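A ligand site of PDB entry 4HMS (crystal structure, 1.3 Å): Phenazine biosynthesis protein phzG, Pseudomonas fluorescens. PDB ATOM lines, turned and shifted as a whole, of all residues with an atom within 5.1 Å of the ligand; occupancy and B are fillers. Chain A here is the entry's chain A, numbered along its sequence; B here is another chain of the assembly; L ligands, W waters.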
ATOM      1  N   GLU A  58     -11.122   5.325 -21.019  1.00  0.00           N
ATOM      2  CA  GLU A  58     -11.862   4.431 -20.112  1.00  0.00           C
ATOM      3  C   GLU A  58     -11.065   4.020 -18.860  1.00  0.00           C
ATOM      4  O   GLU A  58     -10.844   2.830 -18.585  1.00  0.00           O
ATOM      5  CB  GLU A  58     -12.437   3.241 -20.844  1.00  0.00           C
ATOM      6  CG  GLU A  58     -13.465   3.594 -21.915  1.00  0.00           C
ATOM      7  CD  GLU A  58     -14.032   2.367 -22.575  1.00  0.00           C
ATOM      8  OE1 GLU A  58     -14.312   1.368 -21.861  1.00  0.00           O
ATOM      9  OE2 GLU A  58     -14.263   2.402 -23.806  1.00  0.00           O
ATOM     10  N   ALA A  61     -12.747   1.374 -16.191  1.00  0.00           N
ATOM     11  CA  ALA A  61     -13.095   0.030 -16.623  1.00  0.00           C
ATOM     12  C   ALA A  61     -12.345  -0.985 -15.723  1.00  0.00           C
ATOM     13  O   ALA A  61     -11.152  -1.231 -15.899  1.00  0.00           O
ATOM     14  CB  ALA A  61     -12.761  -0.182 -18.093  1.00  0.00           C
ATOM     15  N   THR A  75     -14.233 -13.470 -13.714  1.00  0.00           N
ATOM     16  CA  THR A  75     -13.903 -12.073 -14.034  1.00  0.00           C
ATOM     17  C   THR A  75     -14.825 -11.496 -15.086  1.00  0.00           C
ATOM     18  O   THR A  75     -15.406 -12.274 -15.896  1.00  0.00           O
ATOM     19  CB  THR A  75     -12.443 -11.921 -14.494  1.00  0.00           C
ATOM     20  OG1 THR A  75     -12.195 -12.746 -15.648  1.00  0.00           O
ATOM     21  CG2 THR A  75     -11.447 -12.237 -13.366  1.00  0.00           C
ATOM     22  N   ARG A  76     -14.867 -10.150 -15.129  1.00  0.00           N
ATOM     23  CA  ARG A  76     -15.566  -9.375 -16.172  1.00  0.00           C
ATOM     24  C   ARG A  76     -15.243  -7.928 -15.925  1.00  0.00           C
ATOM     25  O   ARG A  76     -14.812  -7.588 -14.812  1.00  0.00           O
ATOM     26  CB  ARG A  76     -17.098  -9.557 -16.142  1.00  0.00           C
ATOM     27  CG  ARG A  76     -17.790  -8.871 -14.969  1.00  0.00           C
ATOM     28  CD  ARG A  76     -17.463  -9.439 -13.605  1.00  0.00           C
ATOM     29  NE  ARG A  76     -17.903 -10.809 -13.481  1.00  0.00           N
ATOM     30  CZ  ARG A  76     -17.643 -11.636 -12.483  1.00  0.00           C
ATOM     31  NH1 ARG A  76     -18.288 -12.797 -12.419  1.00  0.00           N
ATOM     32  NH2 ARG A  76     -16.764 -11.343 -11.540  1.00  0.00           N
ATOM     33  N   ILE A  77     -15.488  -7.061 -16.926  1.00  0.00           N
ATOM     34  CA  ILE A  77     -15.359  -5.648 -16.737  1.00  0.00           C
ATOM     35  C   ILE A  77     -16.670  -5.067 -16.146  1.00  0.00           C
ATOM     36  O   ILE A  77     -17.776  -5.351 -16.599  1.00  0.00           O
ATOM     37  CB  ILE A  77     -15.054  -4.928 -18.045  1.00  0.00           C
ATOM     38  CG1 ILE A  77     -13.744  -5.427 -18.650  1.00  0.00           C
ATOM     39  CG2 ILE A  77     -14.976  -3.438 -17.801  1.00  0.00           C
ATOM     40  CD1 ILE A  77     -12.436  -5.178 -17.881  1.00  0.00           C
ATOM     41  N   VAL A  78     -16.553  -4.206 -15.135  1.00  0.00           N
ATOM     42  CA  VAL A  78     -17.631  -3.320 -14.690  1.00  0.00           C
ATOM     43  C   VAL A  78     -17.057  -1.899 -14.604  1.00  0.00           C
ATOM     44  O   VAL A  78     -15.817  -1.713 -14.518  1.00  0.00           O
ATOM     45  CB  VAL A  78     -18.275  -3.704 -13.332  1.00  0.00           C
ATOM     46  CG1 VAL A  78     -18.884  -5.123 -13.407  1.00  0.00           C
ATOM     47  CG2 VAL A  78     -17.249  -3.601 -12.188  1.00  0.00           C
ATOM     48  N   VAL A  79     -17.922  -0.883 -14.629  1.00  0.00           N
ATOM     49  CA  VAL A  79     -17.475   0.500 -14.509  1.00  0.00           C
ATOM     50  C   VAL A  79     -17.610   1.007 -13.071  1.00  0.00           C
ATOM     51  O   VAL A  79     -18.628   0.799 -12.418  1.00  0.00           O
ATOM     52  CB  VAL A  79     -18.275   1.430 -15.442  1.00  0.00           C
ATOM     53  CG1 VAL A  79     -17.881   2.866 -15.228  1.00  0.00           C
ATOM     54  CG2 VAL A  79     -18.111   1.023 -16.884  1.00  0.00           C
ATOM     55  N   SER A  91     -22.606  -0.789 -10.278  1.00  0.00           N
ATOM     56  CA  SER A  91     -23.922  -1.374 -10.360  1.00  0.00           C
ATOM     57  C   SER A  91     -23.929  -2.622 -11.208  1.00  0.00           C
ATOM     58  O   SER A  91     -23.077  -2.794 -12.090  1.00  0.00           O
ATOM     59  CB  SER A  91     -24.906  -0.387 -10.984  1.00  0.00           C
ATOM     60  OG  SER A  91     -25.001   0.792 -10.203  1.00  0.00           O
ATOM     61  N   THR A  92     -24.884  -3.504 -10.955  1.00  0.00           N
ATOM     62  CA  THR A  92     -25.009  -4.745 -11.711  1.00  0.00           C
ATOM     63  C   THR A  92     -26.397  -5.342 -11.460  1.00  0.00           C
ATOM     64  O   THR A  92     -27.281  -4.702 -10.888  1.00  0.00           O
ATOM     65  CB  THR A  92     -23.847  -5.719 -11.390  1.00  0.00           C
ATOM     66  OG1 THR A  92     -23.853  -6.751 -12.364  1.00  0.00           O
ATOM     67  CG2 THR A  92     -23.969  -6.346 -10.001  1.00  0.00           C
ATOM     68  N   HIS A  93     -26.614  -6.580 -11.918  1.00  0.00           N
ATOM     69  CA  HIS A  93     -27.833  -7.318 -11.569  1.00  0.00           C
ATOM     70  C   HIS A  93     -27.554  -8.418 -10.570  1.00  0.00           C
ATOM     71  O   HIS A  93     -26.555  -9.145 -10.679  1.00  0.00           O
ATOM     72  CB  HIS A  93     -28.491  -7.881 -12.830  1.00  0.00           C
ATOM     73  CG  HIS A  93     -28.903  -6.801 -13.764  1.00  0.00           C
ATOM     74  ND1 HIS A  93     -30.175  -6.267 -13.782  1.00  0.00           N
ATOM     75  CD2 HIS A  93     -28.170  -6.053 -14.614  1.00  0.00           C
ATOM     76  CE1 HIS A  93     -30.225  -5.282 -14.664  1.00  0.00           C
ATOM     77  NE2 HIS A  93     -29.013  -5.113 -15.161  1.00  0.00           N
ATOM     78  N   SER A  96     -26.978 -12.033 -11.798  1.00  0.00           N
ATOM     79  CA  SER A  96     -25.823 -12.326 -12.646  1.00  0.00           C
ATOM     80  C   SER A  96     -24.871 -13.280 -11.934  1.00  0.00           C
ATOM     81  O   SER A  96     -25.027 -13.553 -10.731  1.00  0.00           O
ATOM     82  CB  SER A  96     -25.102 -11.058 -12.992  1.00  0.00           C
ATOM     83  OG  SER A  96     -24.491 -10.440 -11.844  1.00  0.00           O
ATOM     84  N   GLN A  97     -23.839 -13.732 -12.645  1.00  0.00           N
ATOM     85  CA  GLN A  97     -22.869 -14.593 -11.971  1.00  0.00           C
ATOM     86  C   GLN A  97     -22.158 -13.870 -10.816  1.00  0.00           C
ATOM     87  O   GLN A  97     -21.983 -14.440  -9.734  1.00  0.00           O
ATOM     88  CB  GLN A  97     -21.856 -15.185 -12.960  1.00  0.00           C
ATOM     89  CG  GLN A  97     -20.850 -16.109 -12.282  1.00  0.00           C
ATOM     90  CD  GLN A  97     -20.001 -16.884 -13.262  1.00  0.00           C
ATOM     91  OE1 GLN A  97     -20.280 -16.961 -14.464  1.00  0.00           O
ATOM     92  NE2 GLN A  97     -19.069 -17.585 -12.740  1.00  0.00           N
ATOM     93  N   LYS A  98     -21.737 -12.627 -11.061  1.00  0.00           N
ATOM     94  CA  LYS A  98     -21.008 -11.890 -10.046  1.00  0.00           C
ATOM     95  C   LYS A  98     -21.935 -11.679  -8.838  1.00  0.00           C
ATOM     96  O   LYS A  98     -21.495 -11.707  -7.683  1.00  0.00           O
ATOM     97  CB  LYS A  98     -20.407 -10.556 -10.576  1.00  0.00           C
ATOM     98  CG  LYS A  98     -21.366  -9.335 -10.577  1.00  0.00           C
ATOM     99  CD  LYS A  98     -20.823  -8.232 -11.458  1.00  0.00           C
ATOM    100  CE  LYS A  98     -20.870  -8.539 -12.971  1.00  0.00           C
ATOM    101  NZ  LYS A  98     -22.252  -8.912 -13.396  1.00  0.00           N
ATOM    102  N   GLY A  99     -23.229 -11.411  -9.085  1.00  0.00           N
ATOM    103  CA  GLY A  99     -24.167 -11.134  -8.009  1.00  0.00           C
ATOM    104  C   GLY A  99     -24.389 -12.382  -7.166  1.00  0.00           C
ATOM    105  O   GLY A  99     -24.430 -12.365  -5.913  1.00  0.00           O
ATOM    106  N   GLN A 155     -29.717 -10.813 -16.683  1.00  0.00           N
ATOM    107  CA  GLN A 155     -28.284 -10.876 -16.994  1.00  0.00           C
ATOM    108  C   GLN A 155     -27.677 -12.238 -16.626  1.00  0.00           C
ATOM    109  O   GLN A 155     -27.785 -12.687 -15.498  1.00  0.00           O
ATOM    110  CB  GLN A 155     -27.600  -9.724 -16.255  1.00  0.00           C
ATOM    111  CG  GLN A 155     -26.144  -9.546 -16.578  1.00  0.00           C
ATOM    112  CD  GLN A 155     -25.547  -8.350 -15.923  1.00  0.00           C
ATOM    113  OE1 GLN A 155     -25.392  -8.310 -14.697  1.00  0.00           O
ATOM    114  NE2 GLN A 155     -25.223  -7.334 -16.718  1.00  0.00           N
ATOM    115  N   SER A 156     -26.999 -12.814 -17.604  1.00  0.00           N
ATOM    116  CA  SER A 156     -26.171 -14.022 -17.462  1.00  0.00           C
ATOM    117  C   SER A 156     -26.935 -15.346 -17.509  1.00  0.00           C
ATOM    118  O   SER A 156     -26.320 -16.400 -17.569  1.00  0.00           O
ATOM    119  CB  SER A 156     -25.208 -13.973 -16.257  1.00  0.00           C
ATOM    120  OG  SER A 156     -24.540 -12.705 -16.294  1.00  0.00           O
ATOM    121  N   LEU B  22     -18.761   3.342 -22.902  1.00  0.00           N
ATOM    122  CA  LEU B  22     -18.010   2.706 -24.012  1.00  0.00           C
ATOM    123  C   LEU B  22     -17.631   3.606 -25.156  1.00  0.00           C
ATOM    124  O   LEU B  22     -18.418   4.330 -25.781  1.00  0.00           O
ATOM    125  CB  LEU B  22     -18.656   1.410 -24.555  1.00  0.00           C
ATOM    126  CG  LEU B  22     -18.340   0.261 -23.592  1.00  0.00           C
ATOM    127  CD1 LEU B  22     -18.763   0.555 -22.192  1.00  0.00           C
ATOM    128  CD2 LEU B  22     -18.761  -1.082 -24.097  1.00  0.00           C
ATOM    129  N   TYR B 113      -9.823  -7.033 -22.428  1.00  0.00           N
ATOM    130  CA  TYR B 113     -10.800  -6.032 -22.809  1.00  0.00           C
ATOM    131  C   TYR B 113     -10.136  -5.065 -23.794  1.00  0.00           C
ATOM    132  O   TYR B 113      -9.078  -4.480 -23.493  1.00  0.00           O
ATOM    133  CB  TYR B 113     -11.341  -5.239 -21.584  1.00  0.00           C
ATOM    134  CG  TYR B 113     -12.205  -4.052 -21.978  1.00  0.00           C
ATOM    135  CD1 TYR B 113     -13.211  -4.205 -22.944  1.00  0.00           C
ATOM    136  CD2 TYR B 113     -12.022  -2.782 -21.423  1.00  0.00           C
ATOM    137  CE1 TYR B 113     -13.974  -3.132 -23.363  1.00  0.00           C
ATOM    138  CE2 TYR B 113     -12.780  -1.701 -21.818  1.00  0.00           C
ATOM    139  CZ  TYR B 113     -13.757  -1.886 -22.789  1.00  0.00           C
ATOM    140  OH  TYR B 113     -14.520  -0.822 -23.208  1.00  0.00           O
ATOM    141  N   GLN B 120     -14.732  -8.103 -25.072  1.00  0.00           N
ATOM    142  CA  GLN B 120     -14.089  -8.774 -23.941  1.00  0.00           C
ATOM    143  C   GLN B 120     -13.973 -10.262 -24.214  1.00  0.00           C
ATOM    144  O   GLN B 120     -14.835 -10.838 -24.886  1.00  0.00           O
ATOM    145  CB  GLN B 120     -14.909  -8.753 -22.616  1.00  0.00           C
ATOM    146  CG  GLN B 120     -15.432  -7.591 -22.103  1.00  0.00           C
ATOM    147  CD  GLN B 120     -16.161  -7.962 -20.737  1.00  0.00           C
ATOM    148  OE1 GLN B 120     -15.556  -7.991 -19.650  1.00  0.00           O
ATOM    149  NE2 GLN B 120     -17.456  -8.093 -20.833  1.00  0.00           N
ATOM    150  N   GLU B 196     -15.902 -16.984 -22.379  1.00  0.00           N
ATOM    151  CA  GLU B 196     -16.961 -16.123 -22.922  1.00  0.00           C
ATOM    152  C   GLU B 196     -16.344 -15.116 -23.875  1.00  0.00           C
ATOM    153  O   GLU B 196     -15.338 -14.460 -23.550  1.00  0.00           O
ATOM    154  CB  GLU B 196     -17.754 -15.413 -21.828  1.00  0.00           C
ATOM    155  CG  GLU B 196     -18.820 -14.504 -22.441  1.00  0.00           C
ATOM    156  CD  GLU B 196     -19.627 -13.700 -21.457  1.00  0.00           C
ATOM    157  OE1 GLU B 196     -19.850 -14.157 -20.290  1.00  0.00           O
ATOM    158  OE2 GLU B 196     -20.052 -12.579 -21.838  1.00  0.00           O
ATOM    159  N   TRP B 198     -17.483 -11.621 -25.634  1.00  0.00           N
ATOM    160  CA  TRP B 198     -18.468 -10.562 -25.438  1.00  0.00           C
ATOM    161  C   TRP B 198     -18.242  -9.447 -26.450  1.00  0.00           C
ATOM    162  O   TRP B 198     -17.120  -8.948 -26.597  1.00  0.00           O
ATOM    163  CB  TRP B 198     -18.318  -9.977 -24.027  1.00  0.00           C
ATOM    164  CG  TRP B 198     -19.309  -8.958 -23.555  1.00  0.00           C
ATOM    165  CD1 TRP B 198     -20.286  -9.185 -22.642  1.00  0.00           C
ATOM    166  CD2 TRP B 198     -19.396  -7.555 -23.908  1.00  0.00           C
ATOM    167  NE1 TRP B 198     -21.004  -8.034 -22.404  1.00  0.00           N
ATOM    168  CE2 TRP B 198     -20.475  -7.015 -23.150  1.00  0.00           C
ATOM    169  CE3 TRP B 198     -18.687  -6.706 -24.755  1.00  0.00           C
ATOM    170  CZ2 TRP B 198     -20.845  -5.678 -23.214  1.00  0.00           C
ATOM    171  CZ3 TRP B 198     -19.105  -5.365 -24.832  1.00  0.00           C
ATOM    172  CH2 TRP B 198     -20.159  -4.868 -24.061  1.00  0.00           C
ATOM    173  N   ARG B 208     -23.106 -12.327 -26.172  1.00  0.00           N
ATOM    174  CA  ARG B 208     -22.335 -13.109 -25.203  1.00  0.00           C
ATOM    175  C   ARG B 208     -22.361 -14.572 -25.628  1.00  0.00           C
ATOM    176  O   ARG B 208     -23.412 -15.224 -25.600  1.00  0.00           O
ATOM    177  CB  ARG B 208     -22.954 -12.993 -23.823  1.00  0.00           C
ATOM    178  CG  ARG B 208     -23.026 -11.563 -23.314  1.00  0.00           C
ATOM    179  CD  ARG B 208     -23.552 -11.457 -21.898  1.00  0.00           C
ATOM    180  NE  ARG B 208     -22.650 -12.131 -20.955  1.00  0.00           N
ATOM    181  CZ  ARG B 208     -22.904 -12.297 -19.665  1.00  0.00           C
ATOM    182  NH1 ARG B 208     -24.055 -11.880 -19.137  1.00  0.00           N
ATOM    183  NH2 ARG B 208     -22.021 -12.902 -18.898  1.00  0.00           N
ATOM    184  N   PRO B 225     -27.669 -10.292 -21.857  1.00  0.00           N
ATOM    185  CA  PRO B 225     -26.727  -9.194 -21.583  1.00  0.00           C
ATOM    186  C   PRO B 225     -26.894  -8.568 -20.215  1.00  0.00           C
ATOM    187  O   PRO B 225     -25.904  -7.968 -19.734  1.00  0.00           O
ATOM    188  CB  PRO B 225     -27.057  -8.200 -22.689  1.00  0.00           C
ATOM    189  CG  PRO B 225     -28.453  -8.506 -23.081  1.00  0.00           C
ATOM    190  CD  PRO B 225     -28.604  -9.954 -22.935  1.00  0.00           C
ATOM    191  OXT PRO B 225     -27.967  -8.628 -19.585  1.00  0.00           O
HETATM  192  N1  LIG L   1     -22.008  -5.116 -16.385  1.00  0.00           N
HETATM  193  C1  LIG L   1     -22.559  -4.644 -15.256  1.00  0.00           C
HETATM  194  O1  LIG L   1     -23.412  -5.288 -14.659  1.00  0.00           O
HETATM  195  N2  LIG L   1     -22.166  -3.433 -14.729  1.00  0.00           N
HETATM  196  C2  LIG L   1     -21.241  -2.630 -15.353  1.00  0.00           C
HETATM  197  O2  LIG L   1     -20.918  -1.565 -14.840  1.00  0.00           O
HETATM  198  C3  LIG L   1     -20.718  -3.091 -16.563  1.00  0.00           C
HETATM  199  N3  LIG L   1     -19.825  -2.312 -17.229  1.00  0.00           N
HETATM  200  C4  LIG L   1     -19.228  -2.824 -18.381  1.00  0.00           C
HETATM  201  C5  LIG L   1     -18.217  -2.092 -19.039  1.00  0.00           C
HETATM  202  C6  LIG L   1     -17.570  -2.558 -20.173  1.00  0.00           C
HETATM  203  C7  LIG L   1     -16.494  -1.761 -20.817  1.00  0.00           C
HETATM  204  C8  LIG L   1     -17.915  -3.806 -20.658  1.00  0.00           C
HETATM  205  C9  LIG L   1     -17.266  -4.385 -21.874  1.00  0.00           C
HETATM  206  C10 LIG L   1     -18.911  -4.556 -20.028  1.00  0.00           C
HETATM  207  C11 LIG L   1     -19.562  -4.082 -18.874  1.00  0.00           C
HETATM  208  N4  LIG L   1     -20.555  -4.815 -18.211  1.00  0.00           N
HETATM  209  C12 LIG L   1     -21.088  -4.340 -17.034  1.00  0.00           C
HETATM  210  C13 LIG L   1     -20.915  -6.209 -18.651  1.00  0.00           C
HETATM  211  C14 LIG L   1     -20.072  -7.201 -17.817  1.00  0.00           C
HETATM  212  O3  LIG L   1     -18.742  -7.258 -18.323  1.00  0.00           O
HETATM  213  C15 LIG L   1     -20.652  -8.617 -17.841  1.00  0.00           C
HETATM  214  O4  LIG L   1     -20.965  -9.040 -19.179  1.00  0.00           O
HETATM  215  C16 LIG L   1     -21.979  -8.711 -17.056  1.00  0.00           C
HETATM  216  O5  LIG L   1     -21.980  -7.828 -15.910  1.00  0.00           O
HETATM  217  C17 LIG L   1     -22.225 -10.134 -16.632  1.00  0.00           C
HETATM  218  O6  LIG L   1     -21.113 -10.600 -15.860  1.00  0.00           O
HETATM  219  P1  LIG L   1     -21.235 -11.991 -15.044  1.00  0.00           P
HETATM  220  O7  LIG L   1     -21.928 -11.671 -13.749  1.00  0.00           O
HETATM  221  O8  LIG L   1     -22.004 -12.984 -15.917  1.00  0.00           O
HETATM  222  O9  LIG L   1     -19.791 -12.421 -14.864  1.00  0.00           O
HETATM  223  O   HOH W   1     -23.281  -8.013 -20.624  1.00  0.00           O
HETATM  224  O   HOH W   2     -17.357 -14.077 -15.478  1.00  0.00           O
HETATM  225  O   HOH W   3     -18.919 -12.595 -17.597  1.00  0.00           O
HETATM  226  O   HOH W   4     -19.179 -10.884 -19.691  1.00  0.00           O
HETATM  227  O   HOH W   5     -21.303   0.176 -12.679  1.00  0.00           O
HETATM  228  O   HOH W   6     -21.379 -15.552 -16.511  1.00  0.00           O
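OE1 of Glu 58 touches C7 of the ligand, at 3.95 Å.
CA of Val 78 touches N3 of the ligand (3.5 Å).
CD1 of Leu 22 of chain B touches C7 of the ligand, at 3.5 Å.
OH of Tyr 113 of chain B touches C7 of the ligand (3.2 Å).
Hydrophobic or aromatic side chains that line the ligand: Ile 77, Val 78, Val 79, Leu 22 of chain B, Tyr 113 of chain B and Trp 198 of chain B.
The side-chain hydroxyl (OG) of Ser 156 sits at hydrogen-bond distance from the guanidinium group (NH1) of Arg 208 of chain B (3.0 Å).
N of Ile 77 sits at hydrogen-bond distance from OE1 of Gln 120 of chain B, at 2.9 Å.
The side-chain hydroxyl (OG1) of Thr 92 sits at hydrogen-bond distance from the side-chain amide oxygen (OE1) of Gln 155 (3.2 Å).
N of Trp 198 of chain B sits at hydrogen-bond distance from O of Gln 120 of chain B (2.9 Å).
The guanidinium group (NE) of Arg 208 of chain B lies within salt-bridge range of the side-chain carboxylate (OE2) of Glu 196 of chain B (2.8 Å).
The side-chain carboxylate of Glu 58 lies within hydrogen-bond range of the side-chain hydroxyl of Tyr 113 of chain B.
O of His 93 is in hydrogen-bond range of OG of Ser 96, 2.7 Å away.
The backbone NH (N) of His 93 lies within hydrogen-bond range of the side-chain amide oxygen (OE1) of Gln 155 (3.5 Å).
Water W4 lies within hydrogen-bond range of O4 of the ligand (2.6 Å), OE2 of Glu 196 of chain B (2.9 Å) and NE2 of Gln 120 of chain B (3.5 Å).
Water W6 bridges O8 of the ligand and OE1 of Gln 97.
Water W5 lies within hydrogen-bond range of the backbone carbonyl oxygen (O) of Val 79 (2.8 Å), an oxygen (O2) of the ligand (2.8 Å) and the backbone NH (N) of Ser 91 (2.9 Å).
Water W3 lies within hydrogen-bond range of O9 of the ligand (2.9 Å), OE1 of Glu 196 of chain B (3.2 Å) and NH2 of Arg 208 of chain B (3.4 Å).
Water W1 lies within hydrogen-bond range of the chain-end carboxylate of Pro 225 of chain B (2.8 Å), the indole nitrogen of Trp 198 of chain B (2.9 Å) and an oxygen (O4) of the ligand (2.9 Å).
Water W2 lies within hydrogen-bond range of O of Thr 75, O9 of the ligand and NH1 of Arg 76.
The side-chain hydroxyl (OG) of Ser 156 sits at hydrogen-bond distance from an oxygen (O8) of the ligand (2.6 Å).
An oxygen (O3) of the ligand is in hydrogen-bond range of the backbone carbonyl oxygen of Ile 77 (2.7 Å).
An oxygen (O7) of the ligand is in hydrogen-bond range of the backbone NH (N) of Lys 98, 2.9 Å away.
O7 of the ligand is in salt-bridge range of NZ of Lys 98, at 2.8 Å.
The side-chain hydroxyl of Thr 92 sits at hydrogen-bond distance from an oxygen (O1) of the ligand (2.8 Å).
The guanidinium group of Arg 76 is in salt-bridge range of an oxygen (O9) of the ligand.
O of Ser 91 lies within hydrogen-bond range of N2 of the ligand (2.9 Å).
The side-chain amide nitrogen of Gln 120 of chain B sits at hydrogen-bond distance from an oxygen (O3) of the ligand.
NH2 of Arg 208 of chain B is in salt-bridge range of O8 of the ligand (3.0 Å).
An oxygen (O7) of the ligand is in hydrogen-bond range of the backbone NH (N) of Gln 97, 3.0 Å away.
The backbone NH (N) of Val 79 lies within hydrogen-bond range of an oxygen (O2) of the ligand.
OG of Ser 96 lies close to O7 of the ligand (3.4 Å).
NE1 of Trp 198 of chain B sits at hydrogen-bond distance from O4 of the ligand (3.4 Å).
The side-chain amide nitrogen of Gln 155 is in hydrogen-bond range of an oxygen (O5) of the ligand.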
